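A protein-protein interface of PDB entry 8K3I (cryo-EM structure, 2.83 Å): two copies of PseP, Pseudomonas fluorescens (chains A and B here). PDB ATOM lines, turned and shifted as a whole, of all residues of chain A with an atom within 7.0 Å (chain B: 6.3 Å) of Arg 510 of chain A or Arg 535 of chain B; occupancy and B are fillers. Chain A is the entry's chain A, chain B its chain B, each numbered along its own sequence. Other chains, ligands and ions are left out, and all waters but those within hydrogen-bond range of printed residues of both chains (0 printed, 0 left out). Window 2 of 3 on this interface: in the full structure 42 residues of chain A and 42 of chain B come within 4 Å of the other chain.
NH1 of Arg 535 of chain A lies close to NH1 of Arg 535 of chain B, at 3.4 Å. The side-chain carboxylate (OD2) of Asp 506 of chain B lies within salt-bridge range of the guanidinium group (NH2) of Arg 535 of chain A (2.7 Å). The guanidinium group (NH2) of Arg 535 of chain B lies within salt-bridge range of the side-chain carboxylate (OD2) of Asp 506 of chain A.
The side-chain carboxylate (OD2) of Asp 506 of chain B is in salt-bridge range of the guanidinium group (NH2) of Arg 510 of chain B. The guanidinium group of Arg 535 of chain B lies within salt-bridge range of the side-chain carboxylate of Asp 506 of chain B, 3.5 Å away. OD1 of Asp 506 of chain A is in salt-bridge range of NH1 of Arg 535 of chain A. The side-chain hydroxyl (OG) of Ser 658 of chain A is in hydrogen-bond range of the backbone carbonyl oxygen (O) of Phe 654 of chain A, at 3.1 Å. NH2 of Arg 510 of chain A lies within salt-bridge range of OD2 of Asp 506 of chain A, at 3.0 Å.
Among the printed residues, merely in contact across the chains: Ser 658 of chain A with Trp 534 of chain B (3.1 Å), Arg 510 of chain A with Trp 534 of chain B (3.1 Å), Ser 658 of chain A with Ser 502 of chain B (3.2 Å), Phe 654 of chain A with Trp 534 of chain B (3.5 Å), Arg 535 of chain A with Arg 510 of chain B (3.8 Å) and Arg 510 of chain A with Arg 535 of chain B (3.8 Å).
Of the printed residues of chain B, Phe 654 of chain A touches Trp 534. Of the printed residues of chain A, Asp 506 of chain B touches Arg 535 (2.7 Å). Of the printed residues of chain A, Arg 510 of chain B touches Arg 535. Of chain A, only Asp 506 (2.7 Å), Arg 510 (3.8 Å) and Arg 535 (3.4 Å) come within 4 Å of Arg 535 of chain B. The nearest printed residue of chain B that does not touch Arg 510 of chain A is Ser 531 of chain B (6.7 Å). The nearest printed residue of chain B that does not touch Phe 654 of chain A is Arg 535 of chain B (5.4 Å).
Hydrophobic or aromatic side chains of chain A within 4 Å of the printed part of chain B: Phe 654. Of the 13 printed residues of chain B, 5 touch a printed residue of chain A. Printed residues of chain B that touch a printed residue of chain A: Ser 502, Asp 506, Arg 510, Trp 534 and Arg 535. Hydrophobic or aromatic side chains of chain B within 4 Å of the printed part of chain A: Trp 534. Among the printed residues, Asp or Glu carboxylates within 4 Å of a Lys or Arg side-chain nitrogen of the other chain: Asp 506 of chain A with Arg 535 of chain B and Arg 535 of chain A with Asp 506 of chain B.
Asp 506 of chain A touches Arg 535 of chain B, and with the chains exchanged Arg 535 of chain A touches Asp 506 of chain B. Arg 510 of chain A touches Arg 535 of chain B, and with the chains exchanged Arg 535 of chain A touches Arg 510 of chain B. Arg 535 of chain B touches its own counterpart, Arg 535 of chain A.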
ATOM      1  N   SER A 503     -24.941  20.874 -19.417  1.00  0.00           N
ATOM      2  CA  SER A 503     -24.073  21.289 -18.324  1.00  0.00           C
ATOM      3  C   SER A 503     -23.924  20.192 -17.283  1.00  0.00           C
ATOM      4  O   SER A 503     -22.830  19.975 -16.759  1.00  0.00           O
ATOM      5  CB  SER A 503     -24.621  22.558 -17.678  1.00  0.00           C
ATOM      6  OG  SER A 503     -24.705  23.607 -18.617  1.00  0.00           O
ATOM      7  N   ALA A 505     -24.222  16.936 -17.778  1.00  0.00           N
ATOM      8  CA  ALA A 505     -23.380  15.889 -18.340  1.00  0.00           C
ATOM      9  C   ALA A 505     -21.911  16.280 -18.287  1.00  0.00           C
ATOM     10  O   ALA A 505     -21.053  15.450 -17.969  1.00  0.00           O
ATOM     11  CB  ALA A 505     -23.808  15.588 -19.774  1.00  0.00           C
ATOM     12  N   ASP A 506     -21.601  17.539 -18.600  1.00  0.00           N
ATOM     13  CA  ASP A 506     -20.215  17.993 -18.518  1.00  0.00           C
ATOM     14  C   ASP A 506     -19.705  17.977 -17.080  1.00  0.00           C
ATOM     15  O   ASP A 506     -18.568  17.570 -16.821  1.00  0.00           O
ATOM     16  CB  ASP A 506     -20.094  19.392 -19.116  1.00  0.00           C
ATOM     17  CG  ASP A 506     -18.663  19.791 -19.371  1.00  0.00           C
ATOM     18  OD1 ASP A 506     -17.804  18.892 -19.463  1.00  0.00           O
ATOM     19  OD2 ASP A 506     -18.394  21.002 -19.480  1.00  0.00           O
ATOM     20  N   PHE A 507     -20.542  18.404 -16.136  1.00  0.00           N
ATOM     21  CA  PHE A 507     -20.128  18.572 -14.749  1.00  0.00           C
ATOM     22  C   PHE A 507     -20.018  17.235 -14.028  1.00  0.00           C
ATOM     23  O   PHE A 507     -19.166  17.063 -13.150  1.00  0.00           O
ATOM     24  CB  PHE A 507     -21.126  19.503 -14.055  1.00  0.00           C
ATOM     25  CG  PHE A 507     -21.197  19.342 -12.566  1.00  0.00           C
ATOM     26  CD1 PHE A 507     -20.193  19.831 -11.753  1.00  0.00           C
ATOM     27  CD2 PHE A 507     -22.290  18.730 -11.978  1.00  0.00           C
ATOM     28  CE1 PHE A 507     -20.268  19.694 -10.382  1.00  0.00           C
ATOM     29  CE2 PHE A 507     -22.368  18.588 -10.612  1.00  0.00           C
ATOM     30  CZ  PHE A 507     -21.355  19.071  -9.813  1.00  0.00           C
ATOM     31  N   ILE A 508     -20.870  16.275 -14.387  1.00  0.00           N
ATOM     32  CA  ILE A 508     -20.889  14.981 -13.714  1.00  0.00           C
ATOM     33  C   ILE A 508     -19.708  14.125 -14.151  1.00  0.00           C
ATOM     34  O   ILE A 508     -19.113  13.405 -13.340  1.00  0.00           O
ATOM     35  CB  ILE A 508     -22.235  14.279 -13.975  1.00  0.00           C
ATOM     36  CG1 ILE A 508     -23.324  14.858 -13.069  1.00  0.00           C
ATOM     37  CG2 ILE A 508     -22.122  12.781 -13.779  1.00  0.00           C
ATOM     38  CD1 ILE A 508     -24.723  14.677 -13.600  1.00  0.00           C
ATOM     39  N   PHE A 509     -19.341  14.190 -15.429  1.00  0.00           N
ATOM     40  CA  PHE A 509     -18.383  13.258 -16.010  1.00  0.00           C
ATOM     41  C   PHE A 509     -16.948  13.772 -15.986  1.00  0.00           C
ATOM     42  O   PHE A 509     -16.136  13.356 -16.823  1.00  0.00           O
ATOM     43  CB  PHE A 509     -18.805  12.905 -17.436  1.00  0.00           C
ATOM     44  CG  PHE A 509     -19.933  11.923 -17.502  1.00  0.00           C
ATOM     45  CD1 PHE A 509     -19.758  10.626 -17.069  1.00  0.00           C
ATOM     46  CD2 PHE A 509     -21.172  12.300 -17.980  1.00  0.00           C
ATOM     47  CE1 PHE A 509     -20.795   9.724 -17.117  1.00  0.00           C
ATOM     48  CE2 PHE A 509     -22.209  11.403 -18.033  1.00  0.00           C
ATOM     49  CZ  PHE A 509     -22.022  10.113 -17.602  1.00  0.00           C
ATOM     50  N   ARG A 510     -16.604  14.657 -15.050  1.00  0.00           N
ATOM     51  CA  ARG A 510     -15.213  15.072 -14.903  1.00  0.00           C
ATOM     52  C   ARG A 510     -14.419  14.050 -14.097  1.00  0.00           C
ATOM     53  O   ARG A 510     -13.492  13.417 -14.614  1.00  0.00           O
ATOM     54  CB  ARG A 510     -15.134  16.445 -14.238  1.00  0.00           C
ATOM     55  CG  ARG A 510     -15.715  17.559 -15.064  1.00  0.00           C
ATOM     56  CD  ARG A 510     -15.075  18.896 -14.728  1.00  0.00           C
ATOM     57  NE  ARG A 510     -15.778  19.982 -15.395  1.00  0.00           N
ATOM     58  CZ  ARG A 510     -15.689  20.247 -16.689  1.00  0.00           C
ATOM     59  NH1 ARG A 510     -14.864  19.579 -17.478  1.00  0.00           N
ATOM     60  NH2 ARG A 510     -16.455  21.198 -17.208  1.00  0.00           N
ATOM     61  N   ASP A 511     -14.777  13.874 -12.832  1.00  0.00           N
ATOM     62  CA  ASP A 511     -14.167  12.879 -11.960  1.00  0.00           C
ATOM     63  C   ASP A 511     -15.251  11.851 -11.654  1.00  0.00           C
ATOM     64  O   ASP A 511     -15.970  11.960 -10.659  1.00  0.00           O
ATOM     65  CB  ASP A 511     -13.609  13.513 -10.693  1.00  0.00           C
ATOM     66  N   ASN A 512     -15.369  10.855 -12.527  1.00  0.00           N
ATOM     67  CA  ASN A 512     -16.405   9.833 -12.420  1.00  0.00           C
ATOM     68  C   ASN A 512     -15.732   8.468 -12.387  1.00  0.00           C
ATOM     69  O   ASN A 512     -15.265   7.978 -13.428  1.00  0.00           O
ATOM     70  CB  ASN A 512     -17.389   9.929 -13.577  1.00  0.00           C
ATOM     71  CG  ASN A 512     -18.779   9.483 -13.194  1.00  0.00           C
ATOM     72  OD1 ASN A 512     -19.055   9.192 -12.033  1.00  0.00           O
ATOM     73  ND2 ASN A 512     -19.664   9.426 -14.171  1.00  0.00           N
ATOM     74  N   PRO A 513     -15.647   7.834 -11.216  1.00  0.00           N
ATOM     75  CA  PRO A 513     -14.965   6.531 -11.137  1.00  0.00           C
ATOM     76  C   PRO A 513     -15.639   5.435 -11.942  1.00  0.00           C
ATOM     77  O   PRO A 513     -14.975   4.461 -12.321  1.00  0.00           O
ATOM     78  CB  PRO A 513     -14.991   6.223  -9.633  1.00  0.00           C
ATOM     79  CG  PRO A 513     -16.165   6.994  -9.120  1.00  0.00           C
ATOM     80  CD  PRO A 513     -16.179   8.260  -9.911  1.00  0.00           C
ATOM     81  N   ARG A 535     -19.683  13.150 -23.599  1.00  0.00           N
ATOM     82  CA  ARG A 535     -18.847  12.963 -22.420  1.00  0.00           C
ATOM     83  C   ARG A 535     -18.594  11.502 -22.071  1.00  0.00           C
ATOM     84  O   ARG A 535     -17.517  11.175 -21.568  1.00  0.00           O
ATOM     85  CB  ARG A 535     -19.483  13.657 -21.212  1.00  0.00           C
ATOM     86  CG  ARG A 535     -20.136  14.984 -21.523  1.00  0.00           C
ATOM     87  CD  ARG A 535     -19.112  16.004 -21.960  1.00  0.00           C
ATOM     88  NE  ARG A 535     -19.727  17.266 -22.344  1.00  0.00           N
ATOM     89  CZ  ARG A 535     -19.053  18.317 -22.786  1.00  0.00           C
ATOM     90  NH1 ARG A 535     -17.738  18.291 -22.908  1.00  0.00           N
ATOM     91  NH2 ARG A 535     -19.716  19.421 -23.115  1.00  0.00           N
ATOM     92  N   PHE A 654     -19.208  25.258 -11.202  1.00  0.00           N
ATOM     93  CA  PHE A 654     -19.315  24.943 -12.621  1.00  0.00           C
ATOM     94  C   PHE A 654     -20.083  26.026 -13.364  1.00  0.00           C
ATOM     95  O   PHE A 654     -19.671  26.456 -14.445  1.00  0.00           O
ATOM     96  CB  PHE A 654     -19.984  23.581 -12.822  1.00  0.00           C
ATOM     97  CG  PHE A 654     -20.134  23.192 -14.267  1.00  0.00           C
ATOM     98  CD1 PHE A 654     -21.242  23.585 -14.997  1.00  0.00           C
ATOM     99  CD2 PHE A 654     -19.158  22.452 -14.900  1.00  0.00           C
ATOM    100  CE1 PHE A 654     -21.367  23.246 -16.319  1.00  0.00           C
ATOM    101  CE2 PHE A 654     -19.285  22.107 -16.222  1.00  0.00           C
ATOM    102  CZ  PHE A 654     -20.389  22.503 -16.931  1.00  0.00           C
ATOM    103  N   SER A 658     -18.552  28.293 -16.406  1.00  0.00           N
ATOM    104  CA  SER A 658     -19.040  28.011 -17.752  1.00  0.00           C
ATOM    105  C   SER A 658     -19.733  29.218 -18.370  1.00  0.00           C
ATOM    106  O   SER A 658     -19.426  29.608 -19.499  1.00  0.00           O
ATOM    107  CB  SER A 658     -19.981  26.812 -17.724  1.00  0.00           C
ATOM    108  OG  SER A 658     -19.265  25.632 -17.436  1.00  0.00           O
ATOM    109  N   SER B 502     -16.121  29.545 -23.071  1.00  0.00           N
ATOM    110  CA  SER B 502     -16.296  28.182 -22.575  1.00  0.00           C
ATOM    111  C   SER B 502     -16.735  27.239 -23.697  1.00  0.00           C
ATOM    112  O   SER B 502     -16.160  26.155 -23.885  1.00  0.00           O
ATOM    113  CB  SER B 502     -17.308  28.176 -21.430  1.00  0.00           C
ATOM    114  OG  SER B 502     -17.485  26.874 -20.905  1.00  0.00           O
ATOM    115  N   ALA B 505     -13.875  26.726 -26.274  1.00  0.00           N
ATOM    116  CA  ALA B 505     -12.867  25.785 -25.803  1.00  0.00           C
ATOM    117  C   ALA B 505     -13.367  24.352 -25.910  1.00  0.00           C
ATOM    118  O   ALA B 505     -12.651  23.472 -26.409  1.00  0.00           O
ATOM    119  CB  ALA B 505     -12.476  26.117 -24.365  1.00  0.00           C
ATOM    120  N   ASP B 506     -14.609  24.107 -25.479  1.00  0.00           N
ATOM    121  CA  ASP B 506     -15.166  22.761 -25.566  1.00  0.00           C
ATOM    122  C   ASP B 506     -15.258  22.288 -27.012  1.00  0.00           C
ATOM    123  O   ASP B 506     -14.946  21.132 -27.317  1.00  0.00           O
ATOM    124  CB  ASP B 506     -16.542  22.728 -24.904  1.00  0.00           C
ATOM    125  CG  ASP B 506     -17.038  21.324 -24.665  1.00  0.00           C
ATOM    126  OD1 ASP B 506     -16.204  20.398 -24.632  1.00  0.00           O
ATOM    127  OD2 ASP B 506     -18.261  21.144 -24.514  1.00  0.00           O
ATOM    128  N   PHE B 509     -11.549  21.755 -28.591  1.00  0.00           N
ATOM    129  CA  PHE B 509     -10.682  20.711 -28.058  1.00  0.00           C
ATOM    130  C   PHE B 509     -11.312  19.321 -28.091  1.00  0.00           C
ATOM    131  O   PHE B 509     -10.974  18.477 -27.253  1.00  0.00           O
ATOM    132  CB  PHE B 509     -10.243  21.080 -26.642  1.00  0.00           C
ATOM    133  CG  PHE B 509      -9.183  22.137 -26.604  1.00  0.00           C
ATOM    134  CD1 PHE B 509      -7.921  21.881 -27.094  1.00  0.00           C
ATOM    135  CD2 PHE B 509      -9.456  23.393 -26.098  1.00  0.00           C
ATOM    136  CE1 PHE B 509      -6.949  22.853 -27.072  1.00  0.00           C
ATOM    137  CE2 PHE B 509      -8.488  24.367 -26.073  1.00  0.00           C
ATOM    138  CZ  PHE B 509      -7.232  24.097 -26.559  1.00  0.00           C
ATOM    139  N   ARG B 510     -12.209  19.054 -29.041  1.00  0.00           N
ATOM    140  CA  ARG B 510     -12.722  17.698 -29.213  1.00  0.00           C
ATOM    141  C   ARG B 510     -11.763  16.846 -30.037  1.00  0.00           C
ATOM    142  O   ARG B 510     -11.201  15.864 -29.541  1.00  0.00           O
ATOM    143  CB  ARG B 510     -14.098  17.729 -29.877  1.00  0.00           C
ATOM    144  CG  ARG B 510     -15.167  18.367 -29.035  1.00  0.00           C
ATOM    145  CD  ARG B 510     -16.544  17.817 -29.365  1.00  0.00           C
ATOM    146  NE  ARG B 510     -17.573  18.574 -28.664  1.00  0.00           N
ATOM    147  CZ  ARG B 510     -17.810  18.486 -27.365  1.00  0.00           C
ATOM    148  NH1 ARG B 510     -17.176  17.611 -26.603  1.00  0.00           N
ATOM    149  NH2 ARG B 510     -18.698  19.304 -26.813  1.00  0.00           N
ATOM    150  N   GLN B 530      -9.997  29.267 -16.540  1.00  0.00           N
ATOM    151  CA  GLN B 530     -10.422  27.989 -15.976  1.00  0.00           C
ATOM    152  C   GLN B 530     -11.230  27.172 -16.979  1.00  0.00           C
ATOM    153  O   GLN B 530     -11.063  25.950 -17.066  1.00  0.00           O
ATOM    154  CB  GLN B 530     -11.221  28.220 -14.694  1.00  0.00           C
ATOM    155  CG  GLN B 530     -11.626  26.948 -13.959  1.00  0.00           C
ATOM    156  CD  GLN B 530     -10.445  26.102 -13.533  1.00  0.00           C
ATOM    157  OE1 GLN B 530      -9.959  26.223 -12.415  1.00  0.00           O
ATOM    158  NE2 GLN B 530      -9.991  25.227 -14.417  1.00  0.00           N
ATOM    159  N   SER B 531     -12.111  27.820 -17.745  1.00  0.00           N
ATOM    160  CA  SER B 531     -12.888  27.091 -18.742  1.00  0.00           C
ATOM    161  C   SER B 531     -11.985  26.510 -19.819  1.00  0.00           C
ATOM    162  O   SER B 531     -12.243  25.415 -20.330  1.00  0.00           O
ATOM    163  CB  SER B 531     -13.943  28.001 -19.363  1.00  0.00           C
ATOM    164  OG  SER B 531     -13.364  28.913 -20.268  1.00  0.00           O
ATOM    165  N   ILE B 532     -10.927  27.233 -20.189  1.00  0.00           N
ATOM    166  CA  ILE B 532      -9.982  26.682 -21.155  1.00  0.00           C
ATOM    167  C   ILE B 532      -9.175  25.543 -20.540  1.00  0.00           C
ATOM    168  O   ILE B 532      -8.970  24.504 -21.175  1.00  0.00           O
ATOM    169  CB  ILE B 532      -9.075  27.793 -21.712  1.00  0.00           C
ATOM    170  CG1 ILE B 532      -9.867  28.677 -22.665  1.00  0.00           C
ATOM    171  CG2 ILE B 532      -7.880  27.200 -22.432  1.00  0.00           C
ATOM    172  CD1 ILE B 532      -9.256  30.019 -22.888  1.00  0.00           C
ATOM    173  N   ALA B 533      -8.712  25.709 -19.298  1.00  0.00           N
ATOM    174  CA  ALA B 533      -7.917  24.669 -18.650  1.00  0.00           C
ATOM    175  C   ALA B 533      -8.733  23.423 -18.339  1.00  0.00           C
ATOM    176  O   ALA B 533      -8.150  22.370 -18.065  1.00  0.00           O
ATOM    177  CB  ALA B 533      -7.284  25.199 -17.365  1.00  0.00           C
ATOM    178  N   TRP B 534     -10.062  23.529 -18.356  1.00  0.00           N
ATOM    179  CA  TRP B 534     -10.903  22.344 -18.234  1.00  0.00           C
ATOM    180  C   TRP B 534     -10.620  21.345 -19.349  1.00  0.00           C
ATOM    181  O   TRP B 534     -10.679  20.130 -19.134  1.00  0.00           O
ATOM    182  CB  TRP B 534     -12.374  22.745 -18.265  1.00  0.00           C
ATOM    183  CG  TRP B 534     -12.966  23.057 -16.943  1.00  0.00           C
ATOM    184  CD1 TRP B 534     -12.408  22.853 -15.720  1.00  0.00           C
ATOM    185  CD2 TRP B 534     -14.252  23.631 -16.710  1.00  0.00           C
ATOM    186  NE1 TRP B 534     -13.265  23.270 -14.736  1.00  0.00           N
ATOM    187  CE2 TRP B 534     -14.406  23.754 -15.318  1.00  0.00           C
ATOM    188  CE3 TRP B 534     -15.288  24.058 -17.544  1.00  0.00           C
ATOM    189  CZ2 TRP B 534     -15.555  24.278 -14.743  1.00  0.00           C
ATOM    190  CZ3 TRP B 534     -16.422  24.577 -16.973  1.00  0.00           C
ATOM    191  CH2 TRP B 534     -16.551  24.681 -15.585  1.00  0.00           C
ATOM    192  N   ARG B 535     -10.318  21.838 -20.547  1.00  0.00           N
ATOM    193  CA  ARG B 535     -10.209  21.014 -21.744  1.00  0.00           C
ATOM    194  C   ARG B 535      -8.777  20.668 -22.125  1.00  0.00           C
ATOM    195  O   ARG B 535      -8.532  19.581 -22.653  1.00  0.00           O
ATOM    196  CB  ARG B 535     -10.880  21.719 -22.927  1.00  0.00           C
ATOM    197  CG  ARG B 535     -12.153  22.455 -22.579  1.00  0.00           C
ATOM    198  CD  ARG B 535     -13.233  21.497 -22.140  1.00  0.00           C
ATOM    199  NE  ARG B 535     -14.443  22.189 -21.722  1.00  0.00           N
ATOM    200  CZ  ARG B 535     -15.530  21.581 -21.271  1.00  0.00           C
ATOM    201  NH1 ARG B 535     -15.592  20.265 -21.173  1.00  0.00           N
ATOM    202  NH2 ARG B 535     -16.579  22.311 -20.909  1.00  0.00           N
ATOM    203  N   HIS B 536      -7.826  21.564 -21.893  1.00  0.00           N
ATOM    204  CA  HIS B 536      -6.459  21.380 -22.353  1.00  0.00           C
ATOM    205  C   HIS B 536      -5.495  22.018 -21.366  1.00  0.00           C
ATOM    206  O   HIS B 536      -5.855  22.984 -20.684  1.00  0.00           O
ATOM    207  CB  HIS B 536      -6.266  22.000 -23.747  1.00  0.00           C
ATOM    208  CG  HIS B 536      -5.151  21.391 -24.535  1.00  0.00           C
ATOM    209  ND1 HIS B 536      -5.186  20.093 -24.995  1.00  0.00           N
ATOM    210  CD2 HIS B 536      -3.966  21.902 -24.942  1.00  0.00           C
ATOM    211  CE1 HIS B 536      -4.070  19.831 -25.650  1.00  0.00           C
ATOM    212  NE2 HIS B 536      -3.313  20.911 -25.633  1.00  0.00           N
ATOM    213  N   PRO B 537      -4.269  21.501 -21.262  1.00  0.00           N
ATOM    214  CA  PRO B 537      -3.258  22.171 -20.435  1.00  0.00           C
ATOM    215  C   PRO B 537      -2.984  23.582 -20.932  1.00  0.00           C
ATOM    216  O   PRO B 537      -3.015  23.860 -22.130  1.00  0.00           O
ATOM    217  CB  PRO B 537      -2.025  21.272 -20.580  1.00  0.00           C
ATOM    218  CG  PRO B 537      -2.303  20.413 -21.767  1.00  0.00           C
ATOM    219  CD  PRO B 537      -3.776  20.214 -21.773  1.00  0.00           C
